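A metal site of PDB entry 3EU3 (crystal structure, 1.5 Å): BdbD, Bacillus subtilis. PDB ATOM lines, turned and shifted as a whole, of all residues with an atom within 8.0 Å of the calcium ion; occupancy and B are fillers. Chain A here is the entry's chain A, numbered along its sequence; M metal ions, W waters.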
ATOM      1  N   ILE A  18     -10.042  -3.738 -25.478  1.00  0.00           N
ATOM      2  CA  ILE A  18     -10.722  -3.622 -26.768  1.00  0.00           C
ATOM      3  C   ILE A  18     -11.665  -4.813 -27.015  1.00  0.00           C
ATOM      4  O   ILE A  18     -12.155  -4.989 -28.124  1.00  0.00           O
ATOM      5  CB  ILE A  18      -9.736  -3.419 -27.941  1.00  0.00           C
ATOM      6  CG1 ILE A  18      -8.794  -4.618 -28.108  1.00  0.00           C
ATOM      7  CG2 ILE A  18      -8.963  -2.086 -27.776  1.00  0.00           C
ATOM      8  CD1 ILE A  18      -8.104  -4.640 -29.470  1.00  0.00           C
ATOM      9  N   LYS A  19     -11.910  -5.613 -25.978  1.00  0.00           N
ATOM     10  CA  LYS A  19     -12.790  -6.762 -26.099  1.00  0.00           C
ATOM     11  C   LYS A  19     -14.172  -6.277 -26.511  1.00  0.00           C
ATOM     12  O   LYS A  19     -14.707  -5.346 -25.903  1.00  0.00           O
ATOM     13  CB  LYS A  19     -12.873  -7.522 -24.776  1.00  0.00           C
ATOM     14  CG  LYS A  19     -13.747  -8.778 -24.841  1.00  0.00           C
ATOM     15  CD  LYS A  19     -13.826  -9.483 -23.487  1.00  0.00           C
ATOM     16  CE  LYS A  19     -12.537 -10.213 -23.179  1.00  0.00           C
ATOM     17  NZ  LYS A  19     -12.656 -11.031 -21.927  1.00  0.00           N
ATOM     18  N   GLY A  20     -14.722  -6.892 -27.563  1.00  0.00           N
ATOM     19  CA  GLY A  20     -16.056  -6.551 -28.062  1.00  0.00           C
ATOM     20  C   GLY A  20     -16.140  -5.243 -28.835  1.00  0.00           C
ATOM     21  O   GLY A  20     -17.247  -4.778 -29.159  1.00  0.00           O
ATOM     22  N   GLN A  21     -14.981  -4.643 -29.106  1.00  0.00           N
ATOM     23  CA  GLN A  21     -14.900  -3.397 -29.904  1.00  0.00           C
ATOM     24  C   GLN A  21     -14.522  -3.659 -31.365  1.00  0.00           C
ATOM     25  O   GLN A  21     -13.864  -4.649 -31.661  1.00  0.00           O
ATOM     26  CB  GLN A  21     -13.838  -2.465 -29.330  1.00  0.00           C
ATOM     27  CG  GLN A  21     -14.032  -2.131 -27.844  1.00  0.00           C
ATOM     28  CD  GLN A  21     -15.288  -1.339 -27.550  1.00  0.00           C
ATOM     29  OE1 GLN A  21     -15.938  -0.831 -28.473  1.00  0.00           O
ATOM     30  NE2 GLN A  21     -15.641  -1.231 -26.259  1.00  0.00           N
ATOM     31  N   PRO A  22     -14.916  -2.738 -32.263  1.00  0.00           N
ATOM     32  CA  PRO A  22     -14.425  -2.852 -33.634  1.00  0.00           C
ATOM     33  C   PRO A  22     -12.892  -2.851 -33.697  1.00  0.00           C
ATOM     34  O   PRO A  22     -12.234  -2.070 -32.999  1.00  0.00           O
ATOM     35  CB  PRO A  22     -14.983  -1.609 -34.307  1.00  0.00           C
ATOM     36  CG  PRO A  22     -16.190  -1.231 -33.470  1.00  0.00           C
ATOM     37  CD  PRO A  22     -15.795  -1.580 -32.067  1.00  0.00           C
ATOM     38  N   SER A  68      -8.563   0.137 -32.854  1.00  0.00           N
ATOM     39  CA  SER A  68      -9.916  -0.054 -32.368  1.00  0.00           C
ATOM     40  C   SER A  68     -10.540   1.314 -32.123  1.00  0.00           C
ATOM     41  O   SER A  68      -9.826   2.253 -31.825  1.00  0.00           O
ATOM     42  CB  SER A  68      -9.882  -0.849 -31.063  1.00  0.00           C
ATOM     43  OG  SER A  68     -11.178  -1.192 -30.624  1.00  0.00           O
ATOM     44  N   PHE A  69     -11.871   1.377 -32.200  1.00  0.00           N
ATOM     45  CA  PHE A  69     -12.615   2.627 -32.025  1.00  0.00           C
ATOM     46  C   PHE A  69     -13.685   2.397 -30.963  1.00  0.00           C
ATOM     47  O   PHE A  69     -14.460   1.442 -31.072  1.00  0.00           O
ATOM     48  CB  PHE A  69     -13.305   3.014 -33.342  1.00  0.00           C
ATOM     49  CG  PHE A  69     -14.116   4.287 -33.266  1.00  0.00           C
ATOM     50  CD1 PHE A  69     -13.493   5.511 -33.421  1.00  0.00           C
ATOM     51  CD2 PHE A  69     -15.494   4.233 -33.051  1.00  0.00           C
ATOM     52  CE1 PHE A  69     -14.228   6.678 -33.369  1.00  0.00           C
ATOM     53  CE2 PHE A  69     -16.242   5.410 -32.990  1.00  0.00           C
ATOM     54  CZ  PHE A  69     -15.613   6.641 -33.142  1.00  0.00           C
ATOM     55  N   VAL A  70     -13.728   3.293 -29.968  1.00  0.00           N
ATOM     56  CA  VAL A  70     -14.718   3.235 -28.888  1.00  0.00           C
ATOM     57  C   VAL A  70     -15.557   4.507 -28.947  1.00  0.00           C
ATOM     58  O   VAL A  70     -15.024   5.594 -29.072  1.00  0.00           O
ATOM     59  CB  VAL A  70     -14.011   3.131 -27.492  1.00  0.00           C
ATOM     60  CG1 VAL A  70     -15.045   3.087 -26.367  1.00  0.00           C
ATOM     61  CG2 VAL A  70     -13.109   1.870 -27.433  1.00  0.00           C
ATOM     62  N   ASN A  71     -16.881   4.359 -28.863  1.00  0.00           N
ATOM     63  CA  ASN A  71     -17.772   5.516 -28.940  1.00  0.00           C
ATOM     64  C   ASN A  71     -17.726   6.360 -27.690  1.00  0.00           C
ATOM     65  O   ASN A  71     -17.714   5.843 -26.575  1.00  0.00           O
ATOM     66  CB  ASN A  71     -19.227   5.066 -29.115  1.00  0.00           C
ATOM     67  CG  ASN A  71     -19.455   4.352 -30.414  1.00  0.00           C
ATOM     68  OD1 ASN A  71     -19.353   4.945 -31.483  1.00  0.00           O
ATOM     69  ND2 ASN A  71     -19.782   3.068 -30.322  1.00  0.00           N
ATOM     70  N   VAL A  72     -17.772   7.669 -27.911  1.00  0.00           N
ATOM     71  CA  VAL A  72     -17.873   8.666 -26.840  1.00  0.00           C
ATOM     72  C   VAL A  72     -19.018   9.599 -27.189  1.00  0.00           C
ATOM     73  O   VAL A  72     -19.096  10.099 -28.320  1.00  0.00           O
ATOM     74  CB  VAL A  72     -16.579   9.464 -26.663  1.00  0.00           C
ATOM     75  CG1 VAL A  72     -16.710  10.445 -25.497  1.00  0.00           C
ATOM     76  CG2 VAL A  72     -15.408   8.512 -26.417  1.00  0.00           C
ATOM     77  N   ALA A  83     -23.645   6.283 -32.806  1.00  0.00           N
ATOM     78  CA  ALA A  83     -23.037   5.182 -32.065  1.00  0.00           C
ATOM     79  C   ALA A  83     -23.866   3.901 -32.182  1.00  0.00           C
ATOM     80  O   ALA A  83     -23.323   2.831 -32.420  1.00  0.00           O
ATOM     81  CB  ALA A  83     -22.808   5.578 -30.606  1.00  0.00           C
ATOM     82  N   SER A  86     -23.348   2.492 -35.604  1.00  0.00           N
ATOM     83  CA  SER A  86     -21.998   1.942 -35.651  1.00  0.00           C
ATOM     84  C   SER A  86     -21.932   0.560 -34.989  1.00  0.00           C
ATOM     85  O   SER A  86     -21.338  -0.370 -35.554  1.00  0.00           O
ATOM     86  CB  SER A  86     -21.027   2.919 -34.988  1.00  0.00           C
ATOM     87  OG  SER A  86     -19.676   2.483 -35.088  1.00  0.00           O
ATOM     88  N   GLU A  87     -22.574   0.430 -33.825  1.00  0.00           N
ATOM     89  CA  GLU A  87     -22.591  -0.851 -33.102  1.00  0.00           C
ATOM     90  C   GLU A  87     -23.303  -1.933 -33.891  1.00  0.00           C
ATOM     91  O   GLU A  87     -22.824  -3.057 -33.986  1.00  0.00           O
ATOM     92  CB  GLU A  87     -23.200  -0.702 -31.713  1.00  0.00           C
ATOM     93  CG  GLU A  87     -22.346   0.114 -30.775  1.00  0.00           C
ATOM     94  CD  GLU A  87     -20.993  -0.552 -30.461  1.00  0.00           C
ATOM     95  OE1 GLU A  87     -20.801  -1.768 -30.706  1.00  0.00           O
ATOM     96  OE2 GLU A  87     -20.110   0.155 -29.931  1.00  0.00           O
ATOM     97  N   TRP A  90     -20.970  -3.142 -36.743  1.00  0.00           N
ATOM     98  CA  TRP A  90     -19.932  -4.024 -36.237  1.00  0.00           C
ATOM     99  C   TRP A  90     -20.483  -5.434 -35.973  1.00  0.00           C
ATOM    100  O   TRP A  90     -19.843  -6.428 -36.290  1.00  0.00           O
ATOM    101  CB  TRP A  90     -19.262  -3.445 -34.979  1.00  0.00           C
ATOM    102  CG  TRP A  90     -18.233  -4.392 -34.460  1.00  0.00           C
ATOM    103  CD1 TRP A  90     -18.277  -5.085 -33.288  1.00  0.00           C
ATOM    104  CD2 TRP A  90     -17.036  -4.813 -35.129  1.00  0.00           C
ATOM    105  NE1 TRP A  90     -17.174  -5.905 -33.171  1.00  0.00           N
ATOM    106  CE2 TRP A  90     -16.389  -5.755 -34.293  1.00  0.00           C
ATOM    107  CE3 TRP A  90     -16.444  -4.479 -36.349  1.00  0.00           C
ATOM    108  CZ2 TRP A  90     -15.177  -6.364 -34.634  1.00  0.00           C
ATOM    109  CZ3 TRP A  90     -15.235  -5.083 -36.698  1.00  0.00           C
ATOM    110  CH2 TRP A  90     -14.622  -6.024 -35.851  1.00  0.00           C
ATOM    111  N   PHE A  97     -17.362  -2.763 -41.652  1.00  0.00           N
ATOM    112  CA  PHE A  97     -17.463  -1.756 -40.611  1.00  0.00           C
ATOM    113  C   PHE A  97     -16.633  -0.490 -40.897  1.00  0.00           C
ATOM    114  O   PHE A  97     -17.116   0.637 -40.751  1.00  0.00           O
ATOM    115  CB  PHE A  97     -17.067  -2.306 -39.243  1.00  0.00           C
ATOM    116  CG  PHE A  97     -17.016  -1.233 -38.196  1.00  0.00           C
ATOM    117  CD1 PHE A  97     -18.188  -0.817 -37.585  1.00  0.00           C
ATOM    118  CD2 PHE A  97     -15.827  -0.568 -37.912  1.00  0.00           C
ATOM    119  CE1 PHE A  97     -18.192   0.216 -36.653  1.00  0.00           C
ATOM    120  CE2 PHE A  97     -15.824   0.472 -36.977  1.00  0.00           C
ATOM    121  CZ  PHE A  97     -16.994   0.854 -36.351  1.00  0.00           C
ATOM    122  N   SER A 147     -27.086  -1.415 -25.184  1.00  0.00           N
ATOM    123  CA  SER A 147     -26.135  -2.013 -24.246  1.00  0.00           C
ATOM    124  C   SER A 147     -24.682  -1.767 -24.668  1.00  0.00           C
ATOM    125  O   SER A 147     -23.810  -1.616 -23.816  1.00  0.00           O
ATOM    126  CB  SER A 147     -26.375  -3.507 -24.062  1.00  0.00           C
ATOM    127  OG  SER A 147     -25.796  -4.237 -25.128  1.00  0.00           O
ATOM    128  N   GLN A 148     -24.444  -1.719 -25.978  1.00  0.00           N
ATOM    129  CA  GLN A 148     -23.084  -1.536 -26.506  1.00  0.00           C
ATOM    130  C   GLN A 148     -22.600  -0.125 -26.306  1.00  0.00           C
ATOM    131  O   GLN A 148     -21.434   0.102 -26.034  1.00  0.00           O
ATOM    132  CB  GLN A 148     -23.011  -1.884 -27.988  1.00  0.00           C
ATOM    133  CG  GLN A 148     -23.236  -3.343 -28.315  1.00  0.00           C
ATOM    134  CD  GLN A 148     -22.284  -4.269 -27.547  1.00  0.00           C
ATOM    135  OE1 GLN A 148     -21.110  -3.945 -27.340  1.00  0.00           O
ATOM    136  NE2 GLN A 148     -22.797  -5.403 -27.108  1.00  0.00           N
ATOM    137  N   VAL A 149     -23.503   0.836 -26.483  1.00  0.00           N
ATOM    138  CA  VAL A 149     -23.189   2.244 -26.260  1.00  0.00           C
ATOM    139  C   VAL A 149     -22.913   2.503 -24.776  1.00  0.00           C
ATOM    140  O   VAL A 149     -22.022   3.270 -24.416  1.00  0.00           O
ATOM    141  CB  VAL A 149     -24.305   3.188 -26.778  1.00  0.00           C
ATOM    142  CG1 VAL A 149     -23.946   4.630 -26.525  1.00  0.00           C
ATOM    143  CG2 VAL A 149     -24.572   2.953 -28.274  1.00  0.00           C
ATOM    144  N   GLU A 150     -23.707   1.878 -23.907  1.00  0.00           N
ATOM    145  CA  GLU A 150     -23.490   2.024 -22.473  1.00  0.00           C
ATOM    146  C   GLU A 150     -22.172   1.390 -22.021  1.00  0.00           C
ATOM    147  O   GLU A 150     -21.482   1.934 -21.160  1.00  0.00           O
ATOM    148  CB  GLU A 150     -24.669   1.455 -21.662  1.00  0.00           C
ATOM    149  CG  GLU A 150     -26.018   2.148 -21.938  1.00  0.00           C
ATOM    150  CD  GLU A 150     -26.047   3.667 -21.669  1.00  0.00           C
ATOM    151  OE1 GLU A 150     -25.142   4.233 -21.025  1.00  0.00           O
ATOM    152  OE2 GLU A 150     -27.030   4.309 -22.117  1.00  0.00           O
ATOM    153  N   LYS A 151     -21.837   0.251 -22.622  1.00  0.00           N
ATOM    154  CA  LYS A 151     -20.540  -0.407 -22.395  1.00  0.00           C
ATOM    155  C   LYS A 151     -19.409   0.549 -22.724  1.00  0.00           C
ATOM    156  O   LYS A 151     -18.449   0.686 -21.954  1.00  0.00           O
ATOM    157  CB  LYS A 151     -20.423  -1.685 -23.241  1.00  0.00           C
ATOM    158  CG  LYS A 151     -18.987  -2.205 -23.416  1.00  0.00           C
ATOM    159  CD  LYS A 151     -18.925  -3.522 -24.161  1.00  0.00           C
ATOM    160  CE  LYS A 151     -17.474  -3.994 -24.264  1.00  0.00           C
ATOM    161  NZ  LYS A 151     -17.375  -5.384 -24.704  1.00  0.00           N
ATOM    162  N   ASP A 152     -19.529   1.230 -23.855  1.00  0.00           N
ATOM    163  CA  ASP A 152     -18.502   2.191 -24.295  1.00  0.00           C
ATOM    164  C   ASP A 152     -18.424   3.363 -23.329  1.00  0.00           C
ATOM    165  O   ASP A 152     -17.340   3.776 -22.959  1.00  0.00           O
ATOM    166  CB  ASP A 152     -18.762   2.708 -25.698  1.00  0.00           C
ATOM    167  CG  ASP A 152     -18.390   1.709 -26.765  1.00  0.00           C
ATOM    168  OD1 ASP A 152     -17.937   0.593 -26.406  1.00  0.00           O
ATOM    169  OD2 ASP A 152     -18.557   2.032 -27.962  1.00  0.00           O
ATOM    170  N   SER A 153     -19.587   3.878 -22.925  1.00  0.00           N
ATOM    171  CA  SER A 153     -19.617   4.941 -21.920  1.00  0.00           C
ATOM    172  C   SER A 153     -18.940   4.539 -20.607  1.00  0.00           C
ATOM    173  O   SER A 153     -18.199   5.325 -20.037  1.00  0.00           O
ATOM    174  CB  SER A 153     -21.056   5.383 -21.671  1.00  0.00           C
ATOM    175  OG  SER A 153     -21.527   6.071 -22.804  1.00  0.00           O
ATOM    176  N   LEU A 155     -16.531   2.377 -20.261  1.00  0.00           N
ATOM    177  CA  LEU A 155     -15.109   2.362 -20.565  1.00  0.00           C
ATOM    178  C   LEU A 155     -14.525   3.783 -20.652  1.00  0.00           C
ATOM    179  O   LEU A 155     -13.438   4.026 -20.108  1.00  0.00           O
ATOM    180  CB  LEU A 155     -14.826   1.569 -21.844  1.00  0.00           C
ATOM    181  CG  LEU A 155     -13.360   1.437 -22.266  1.00  0.00           C
ATOM    182  CD1 LEU A 155     -12.495   0.824 -21.156  1.00  0.00           C
ATOM    183  CD2 LEU A 155     -13.253   0.632 -23.561  1.00  0.00           C
HETATM  184 CA    CA M   1     -18.166  -0.229 -28.833  1.00  0.00          CA
HETATM  185  O   HOH W   1     -19.513  -1.660 -27.154  1.00  0.00           O
HETATM  186  O   HOH W   2     -17.163   1.022 -30.615  1.00  0.00           O
HETATM  187  O   HOH W   3     -18.366  -2.373 -29.834  1.00  0.00           O
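The side-chain carboxylate of Glu 87 sits close to the side-chain amide nitrogen of Asn 71, 3.0 Å away. The side-chain amide nitrogen (ND2) of Asn 71 sits close to the side-chain carboxylate (OD2) of Asp 152.
Asn 71 touches the calcium ion. Within 4 Å of the calcium ion: Gln 21, Asn 71, Glu 87 and Asp 152. The nearest printed residue that does not touch the calcium ion is Pro 22 (4.2 Å).
OE2 of Glu 87 binds the calcium ion, at 2.3 Å. OE1 of Gln 21 binds the calcium ion. The calcium ion is bound by water W3. Water W2 binds the calcium ion, 2.4 Å away. OD2 of Asp 152 is bound to the calcium ion (2.5 Å). The calcium ion is bound by OD1 of Asp 152 (2.6 Å). Water W1 is bound to the calcium ion, at 2.6 Å. The calcium ion has seven donor atoms within binding distance.
Water W2 bridges O of Phe 69 (2.8 Å) and ND2 of Asn 71 (3.3 Å). Water W3 lies within hydrogen-bond range of OE1 of Glu 87 (2.7 Å) and O of Gly 20 (2.7 Å).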
